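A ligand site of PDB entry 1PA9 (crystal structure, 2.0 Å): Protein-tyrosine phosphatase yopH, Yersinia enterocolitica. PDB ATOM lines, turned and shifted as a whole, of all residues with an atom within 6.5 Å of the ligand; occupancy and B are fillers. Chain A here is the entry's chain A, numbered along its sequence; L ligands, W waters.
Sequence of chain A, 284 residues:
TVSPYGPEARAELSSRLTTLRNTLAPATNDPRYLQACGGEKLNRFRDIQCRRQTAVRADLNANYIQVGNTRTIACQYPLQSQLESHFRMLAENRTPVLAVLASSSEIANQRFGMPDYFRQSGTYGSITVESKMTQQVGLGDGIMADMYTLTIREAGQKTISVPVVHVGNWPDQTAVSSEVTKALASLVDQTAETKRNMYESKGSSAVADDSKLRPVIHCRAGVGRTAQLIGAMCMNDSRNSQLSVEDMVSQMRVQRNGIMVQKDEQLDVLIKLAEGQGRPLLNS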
ATOM      1  N   PHE A  45     -18.631  31.157  39.126  1.00  0.00           N
ATOM      2  CA  PHE A  45     -17.284  30.631  39.288  1.00  0.00           C
ATOM      3  C   PHE A  45     -16.457  31.690  40.015  1.00  0.00           C
ATOM      4  O   PHE A  45     -16.249  32.784  39.495  1.00  0.00           O
ATOM      5  CB  PHE A  45     -16.665  30.313  37.925  1.00  0.00           C
ATOM      6  CG  PHE A  45     -17.390  29.216  37.183  1.00  0.00           C
ATOM      7  CD1 PHE A  45     -17.231  27.892  37.567  1.00  0.00           C
ATOM      8  CD2 PHE A  45     -18.253  29.522  36.141  1.00  0.00           C
ATOM      9  CE1 PHE A  45     -17.944  26.876  36.931  1.00  0.00           C
ATOM     10  CE2 PHE A  45     -18.968  28.514  35.499  1.00  0.00           C
ATOM     11  CZ  PHE A  45     -18.809  27.190  35.883  1.00  0.00           C
ATOM     12  N   ASP A  47     -13.422  32.496  40.418  1.00  0.00           N
ATOM     13  CA  ASP A  47     -12.357  33.215  39.716  1.00  0.00           C
ATOM     14  C   ASP A  47     -12.779  33.882  38.406  1.00  0.00           C
ATOM     15  O   ASP A  47     -11.954  34.462  37.713  1.00  0.00           O
ATOM     16  CB  ASP A  47     -11.190  32.258  39.471  1.00  0.00           C
ATOM     17  CG  ASP A  47     -10.572  31.763  40.764  1.00  0.00           C
ATOM     18  OD1 ASP A  47      -9.770  30.807  40.721  1.00  0.00           O
ATOM     19  OD2 ASP A  47     -10.899  32.325  41.834  1.00  0.00           O
ATOM     20  N   ILE A  48     -14.057  33.814  38.086  1.00  0.00           N
ATOM     21  CA  ILE A  48     -14.580  34.422  36.865  1.00  0.00           C
ATOM     22  C   ILE A  48     -15.507  35.533  37.328  1.00  0.00           C
ATOM     23  O   ILE A  48     -16.702  35.320  37.522  1.00  0.00           O
ATOM     24  CB  ILE A  48     -15.373  33.401  36.044  1.00  0.00           C
ATOM     25  CG1 ILE A  48     -14.469  32.204  35.728  1.00  0.00           C
ATOM     26  CG2 ILE A  48     -15.876  34.036  34.750  1.00  0.00           C
ATOM     27  CD1 ILE A  48     -15.161  31.145  34.891  1.00  0.00           C
ATOM     28  N   GLU A 106     -25.411  20.304  29.577  1.00  0.00           N
ATOM     29  CA  GLU A 106     -24.999  21.092  30.737  1.00  0.00           C
ATOM     30  C   GLU A 106     -26.207  21.524  31.569  1.00  0.00           C
ATOM     31  O   GLU A 106     -26.226  21.353  32.782  1.00  0.00           O
ATOM     32  CB  GLU A 106     -24.226  22.332  30.286  1.00  0.00           C
ATOM     33  CG  GLU A 106     -22.826  22.040  29.771  1.00  0.00           C
ATOM     34  CD  GLU A 106     -22.220  23.219  29.052  1.00  0.00           C
ATOM     35  OE1 GLU A 106     -22.578  23.430  27.874  1.00  0.00           O
ATOM     36  OE2 GLU A 106     -21.411  23.944  29.657  1.00  0.00           O
ATOM     37  N   PRO A 171     -20.169  22.054  22.623  1.00  0.00           N
ATOM     38  CA  PRO A 171     -19.472  21.543  23.818  1.00  0.00           C
ATOM     39  C   PRO A 171     -18.645  22.564  24.579  1.00  0.00           C
ATOM     40  O   PRO A 171     -17.897  23.348  23.998  1.00  0.00           O
ATOM     41  CB  PRO A 171     -18.611  20.407  23.257  1.00  0.00           C
ATOM     42  CG  PRO A 171     -19.368  19.943  22.063  1.00  0.00           C
ATOM     43  CD  PRO A 171     -19.812  21.249  21.436  1.00  0.00           C
ATOM     44  N   ASP A 172     -18.786  22.528  25.894  1.00  0.00           N
ATOM     45  CA  ASP A 172     -18.067  23.425  26.795  1.00  0.00           C
ATOM     46  C   ASP A 172     -16.562  23.252  26.562  1.00  0.00           C
ATOM     47  O   ASP A 172     -16.103  22.171  26.202  1.00  0.00           O
ATOM     48  CB  ASP A 172     -18.453  23.058  28.237  1.00  0.00           C
ATOM     49  CG  ASP A 172     -17.795  23.952  29.272  1.00  0.00           C
ATOM     50  OD1 ASP A 172     -17.661  25.172  29.015  1.00  0.00           O
ATOM     51  OD2 ASP A 172     -17.436  23.439  30.348  1.00  0.00           O
ATOM     52  N   GLN A 173     -15.797  24.321  26.740  1.00  0.00           N
ATOM     53  CA  GLN A 173     -14.341  24.267  26.580  1.00  0.00           C
ATOM     54  C   GLN A 173     -13.823  24.005  25.169  1.00  0.00           C
ATOM     55  O   GLN A 173     -12.678  23.574  25.010  1.00  0.00           O
ATOM     56  CB  GLN A 173     -13.767  23.190  27.509  1.00  0.00           C
ATOM     57  CG  GLN A 173     -14.133  23.378  28.960  1.00  0.00           C
ATOM     58  CD  GLN A 173     -13.558  24.655  29.530  1.00  0.00           C
ATOM     59  OE1 GLN A 173     -12.387  24.710  29.935  1.00  0.00           O
ATOM     60  NE2 GLN A 173     -14.362  25.700  29.539  1.00  0.00           N
ATOM     61  N   THR A 174     -14.643  24.255  24.159  1.00  0.00           N
ATOM     62  CA  THR A 174     -14.204  24.026  22.783  1.00  0.00           C
ATOM     63  C   THR A 174     -14.579  25.191  21.894  1.00  0.00           C
ATOM     64  O   THR A 174     -15.259  26.128  22.316  1.00  0.00           O
ATOM     65  CB  THR A 174     -14.850  22.774  22.167  1.00  0.00           C
ATOM     66  OG1 THR A 174     -16.261  22.988  22.013  1.00  0.00           O
ATOM     67  CG2 THR A 174     -14.612  21.547  23.050  1.00  0.00           C
ATOM     68  N   CYS A 219     -22.943  31.694  27.961  1.00  0.00           N
ATOM     69  CA  CYS A 219     -22.746  30.261  27.825  1.00  0.00           C
ATOM     70  C   CYS A 219     -22.851  29.746  29.253  1.00  0.00           C
ATOM     71  O   CYS A 219     -23.920  29.839  29.871  1.00  0.00           O
ATOM     72  CB  CYS A 219     -21.386  29.939  27.180  1.00  0.00           C
ATOM     73  SG  CYS A 219     -19.967  30.965  27.657  1.00  0.00           S
ATOM     74  N   ARG A 220     -21.757  29.218  29.800  1.00  0.00           N
ATOM     75  CA  ARG A 220     -21.784  28.731  31.171  1.00  0.00           C
ATOM     76  C   ARG A 220     -21.119  29.795  32.041  1.00  0.00           C
ATOM     77  O   ARG A 220     -21.745  30.369  32.932  1.00  0.00           O
ATOM     78  CB  ARG A 220     -21.066  27.398  31.262  1.00  0.00           C
ATOM     79  CG  ARG A 220     -21.067  26.723  32.626  1.00  0.00           C
ATOM     80  CD  ARG A 220     -20.901  25.212  32.429  1.00  0.00           C
ATOM     81  NE  ARG A 220     -20.180  24.524  33.495  1.00  0.00           N
ATOM     82  CZ  ARG A 220     -20.555  24.516  34.769  1.00  0.00           C
ATOM     83  NH1 ARG A 220     -21.640  25.159  35.144  1.00  0.00           N
ATOM     84  NH2 ARG A 220     -19.847  23.823  35.661  1.00  0.00           N
ATOM     85  N   ALA A 221     -19.857  30.082  31.755  1.00  0.00           N
ATOM     86  CA  ALA A 221     -19.105  31.085  32.515  1.00  0.00           C
ATOM     87  C   ALA A 221     -19.165  32.439  31.798  1.00  0.00           C
ATOM     88  O   ALA A 221     -18.851  33.473  32.380  1.00  0.00           O
ATOM     89  CB  ALA A 221     -17.657  30.644  32.675  1.00  0.00           C
ATOM     90  N   GLY A 222     -19.558  32.421  30.528  1.00  0.00           N
ATOM     91  CA  GLY A 222     -19.664  33.642  29.765  1.00  0.00           C
ATOM     92  C   GLY A 222     -18.326  34.256  29.367  1.00  0.00           C
ATOM     93  O   GLY A 222     -18.211  35.476  29.252  1.00  0.00           O
ATOM     94  N   VAL A 223     -17.316  33.423  29.151  1.00  0.00           N
ATOM     95  CA  VAL A 223     -15.996  33.918  28.768  1.00  0.00           C
ATOM     96  C   VAL A 223     -15.353  33.129  27.632  1.00  0.00           C
ATOM     97  O   VAL A 223     -14.451  33.617  26.962  1.00  0.00           O
ATOM     98  CB  VAL A 223     -15.030  33.895  29.972  1.00  0.00           C
ATOM     99  CG1 VAL A 223     -15.585  34.765  31.087  1.00  0.00           C
ATOM    100  CG2 VAL A 223     -14.825  32.462  30.451  1.00  0.00           C
ATOM    101  N   GLY A 224     -15.801  31.898  27.426  1.00  0.00           N
ATOM    102  CA  GLY A 224     -15.236  31.074  26.371  1.00  0.00           C
ATOM    103  C   GLY A 224     -16.020  31.137  25.059  1.00  0.00           C
ATOM    104  O   GLY A 224     -15.649  31.862  24.142  1.00  0.00           O
ATOM    105  N   ARG A 225     -17.085  30.355  24.990  1.00  0.00           N
ATOM    106  CA  ARG A 225     -17.932  30.319  23.805  1.00  0.00           C
ATOM    107  C   ARG A 225     -18.546  31.698  23.538  1.00  0.00           C
ATOM    108  O   ARG A 225     -18.607  32.149  22.386  1.00  0.00           O
ATOM    109  CB  ARG A 225     -19.016  29.250  24.003  1.00  0.00           C
ATOM    110  CG  ARG A 225     -18.440  27.836  24.047  1.00  0.00           C
ATOM    111  CD  ARG A 225     -19.420  26.810  24.630  1.00  0.00           C
ATOM    112  NE  ARG A 225     -19.535  26.901  26.076  1.00  0.00           N
ATOM    113  CZ  ARG A 225     -20.261  26.070  26.825  1.00  0.00           C
ATOM    114  NH1 ARG A 225     -20.936  25.079  26.262  1.00  0.00           N
ATOM    115  NH2 ARG A 225     -20.310  26.222  28.144  1.00  0.00           N
ATOM    116  N   THR A 226     -18.992  32.369  24.588  1.00  0.00           N
ATOM    117  CA  THR A 226     -19.567  33.705  24.456  1.00  0.00           C
ATOM    118  C   THR A 226     -18.594  34.678  23.786  1.00  0.00           C
ATOM    119  O   THR A 226     -18.993  35.449  22.901  1.00  0.00           O
ATOM    120  CB  THR A 226     -19.945  34.276  25.847  1.00  0.00           C
ATOM    121  OG1 THR A 226     -21.065  33.561  26.382  1.00  0.00           O
ATOM    122  CG2 THR A 226     -20.282  35.751  25.741  1.00  0.00           C
ATOM    123  N   ILE A 259     -10.353  36.475  31.296  1.00  0.00           N
ATOM    124  CA  ILE A 259     -10.536  35.147  30.720  1.00  0.00           C
ATOM    125  C   ILE A 259     -11.286  35.181  29.377  1.00  0.00           C
ATOM    126  O   ILE A 259     -11.352  34.163  28.687  1.00  0.00           O
ATOM    127  CB  ILE A 259     -11.288  34.191  31.704  1.00  0.00           C
ATOM    128  CG1 ILE A 259     -10.548  34.116  33.046  1.00  0.00           C
ATOM    129  CG2 ILE A 259     -11.366  32.780  31.136  1.00  0.00           C
ATOM    130  CD1 ILE A 259     -10.652  35.367  33.882  1.00  0.00           C
ATOM    131  N   GLN A 262     -11.228  32.213  26.332  1.00  0.00           N
ATOM    132  CA  GLN A 262     -10.530  31.283  27.215  1.00  0.00           C
ATOM    133  C   GLN A 262      -9.526  30.303  26.597  1.00  0.00           C
ATOM    134  O   GLN A 262      -8.405  30.178  27.083  1.00  0.00           O
ATOM    135  CB  GLN A 262     -11.554  30.471  28.016  1.00  0.00           C
ATOM    136  CG  GLN A 262     -10.934  29.329  28.792  1.00  0.00           C
ATOM    137  CD  GLN A 262     -11.959  28.344  29.325  1.00  0.00           C
ATOM    138  OE1 GLN A 262     -12.966  28.054  28.669  1.00  0.00           O
ATOM    139  NE2 GLN A 262     -11.692  27.814  30.509  1.00  0.00           N
ATOM    140  N   GLN A 266     -10.243  28.933  20.582  1.00  0.00           N
ATOM    141  CA  GLN A 266     -11.248  29.967  20.366  1.00  0.00           C
ATOM    142  C   GLN A 266     -10.585  31.216  19.791  1.00  0.00           C
ATOM    143  O   GLN A 266     -11.166  31.892  18.937  1.00  0.00           O
ATOM    144  CB  GLN A 266     -11.969  30.267  21.686  1.00  0.00           C
ATOM    145  CG  GLN A 266     -12.665  29.034  22.259  1.00  0.00           C
ATOM    146  CD  GLN A 266     -13.189  29.218  23.669  1.00  0.00           C
ATOM    147  OE1 GLN A 266     -12.590  29.922  24.483  1.00  0.00           O
ATOM    148  NE2 GLN A 266     -14.290  28.549  23.986  1.00  0.00           N
HETATM  149  S1  LIG L   1     -17.547  28.851  28.925  1.00  0.00           S
HETATM  150  O1  LIG L   1     -16.445  27.708  29.512  1.00  0.00           O
HETATM  151  O2  LIG L   1     -18.814  28.570  29.512  1.00  0.00           O
HETATM  152  O3  LIG L   1     -17.555  28.672  27.486  1.00  0.00           O
HETATM  153  O4  LIG L   1     -17.123  30.171  29.293  1.00  0.00           O
HETATM  154  O5  LIG L   1     -18.003  26.244  31.330  1.00  0.00           O
HETATM  155  O6  LIG L   1     -13.070  29.294  34.254  1.00  0.00           O
HETATM  156  O7  LIG L   1     -12.783  29.864  32.210  1.00  0.00           O
HETATM  157  C1  LIG L   1     -15.024  28.441  31.201  1.00  0.00           C
HETATM  158  N1  LIG L   1     -13.430  29.244  33.050  1.00  0.00           N
HETATM  159  C2  LIG L   1     -16.566  26.958  33.246  1.00  0.00           C
HETATM  160  C3  LIG L   1     -16.233  27.631  30.813  1.00  0.00           C
HETATM  161  C4  LIG L   1     -15.391  27.733  33.631  1.00  0.00           C
HETATM  162  C5  LIG L   1     -16.982  26.898  31.857  1.00  0.00           C
HETATM  163  C6  LIG L   1     -14.601  28.491  32.625  1.00  0.00           C
HETATM  164  O   HOH W   1     -14.955  27.646  26.795  1.00  0.00           O
HETATM  165  O   HOH W   2     -12.928  27.974  37.185  1.00  0.00           O
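OD1 of Asp 172 lies within hydrogen-bond range of O5 of the ligand (2.6 Å).
An oxygen (O2) of the ligand lies within hydrogen-bond range of the backbone NH (N) of Arg 220, 3.0 Å away.
An oxygen (O7) of the ligand is in hydrogen-bond range of the side-chain amide nitrogen of Gln 262 (2.9 Å).
The backbone NH (N) of Val 223 lies within hydrogen-bond range of an oxygen (O4) of the ligand (3.3 Å).
The backbone NH (N) of Ala 221 lies within hydrogen-bond range of an oxygen (O2) of the ligand (2.9 Å).
The side-chain sulfur (SG) of Cys 219 is in hydrogen-bond range of an oxygen (O2) of the ligand (3.2 Å).
An oxygen (O3) of the ligand lies within salt-bridge range of the guanidinium group (NE) of Arg 225, at 3.0 Å.
An oxygen (O4) of the ligand is in hydrogen-bond range of the backbone NH (N) of Gly 224 (2.9 Å).
O1 of the ligand is in hydrogen-bond range of NE2 of Gln 173 (2.9 Å).
N of Arg 225 is in hydrogen-bond range of O3 of the ligand, at 3.0 Å.
N of Arg 225 lies close to NE2 of Gln 266 (3.5 Å).
The backbone NH (N) of Cys 219 is in hydrogen-bond range of the side-chain hydroxyl (OG1) of Thr 226, 3.1 Å away.
The guanidinium group (NH2) of Arg 225 lies within salt-bridge range of the side-chain carboxylate (OD1) of Asp 172.
SG of Cys 219 is in hydrogen-bond range of N of Gly 222 (3.2 Å).
The guanidinium group (NH1) of Arg 225 lies within salt-bridge range of the side-chain carboxylate (OE1) of Glu 106 (2.8 Å).
OE1 of Gln 262 sits at hydrogen-bond distance from NE2 of Gln 173 (2.9 Å).
The backbone NH of Gln 262 lies within hydrogen-bond range of the side-chain amide oxygen of Gln 266.
The side-chain carboxylate (OD1) of Asp 172 lies within hydrogen-bond range of the side-chain amide nitrogen (NE2) of Gln 173 (3.4 Å).
Phe 45 touches the ligand.
Ile 48 touches the ligand.
Gly 222 touches the ligand (N to O4, 3.5 Å).
Ile 259 touches the ligand (CG2 to O7, 3.4 Å).
Hydrophobic or aromatic side chains that line the ligand: Phe 45, Ile 48, Ala 221, Val 223 and Ile 259.
Water W1 lies within hydrogen-bond range of OE1 of Gln 262, O3 of the ligand, NE2 of Gln 266 and NE2 of Gln 173.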
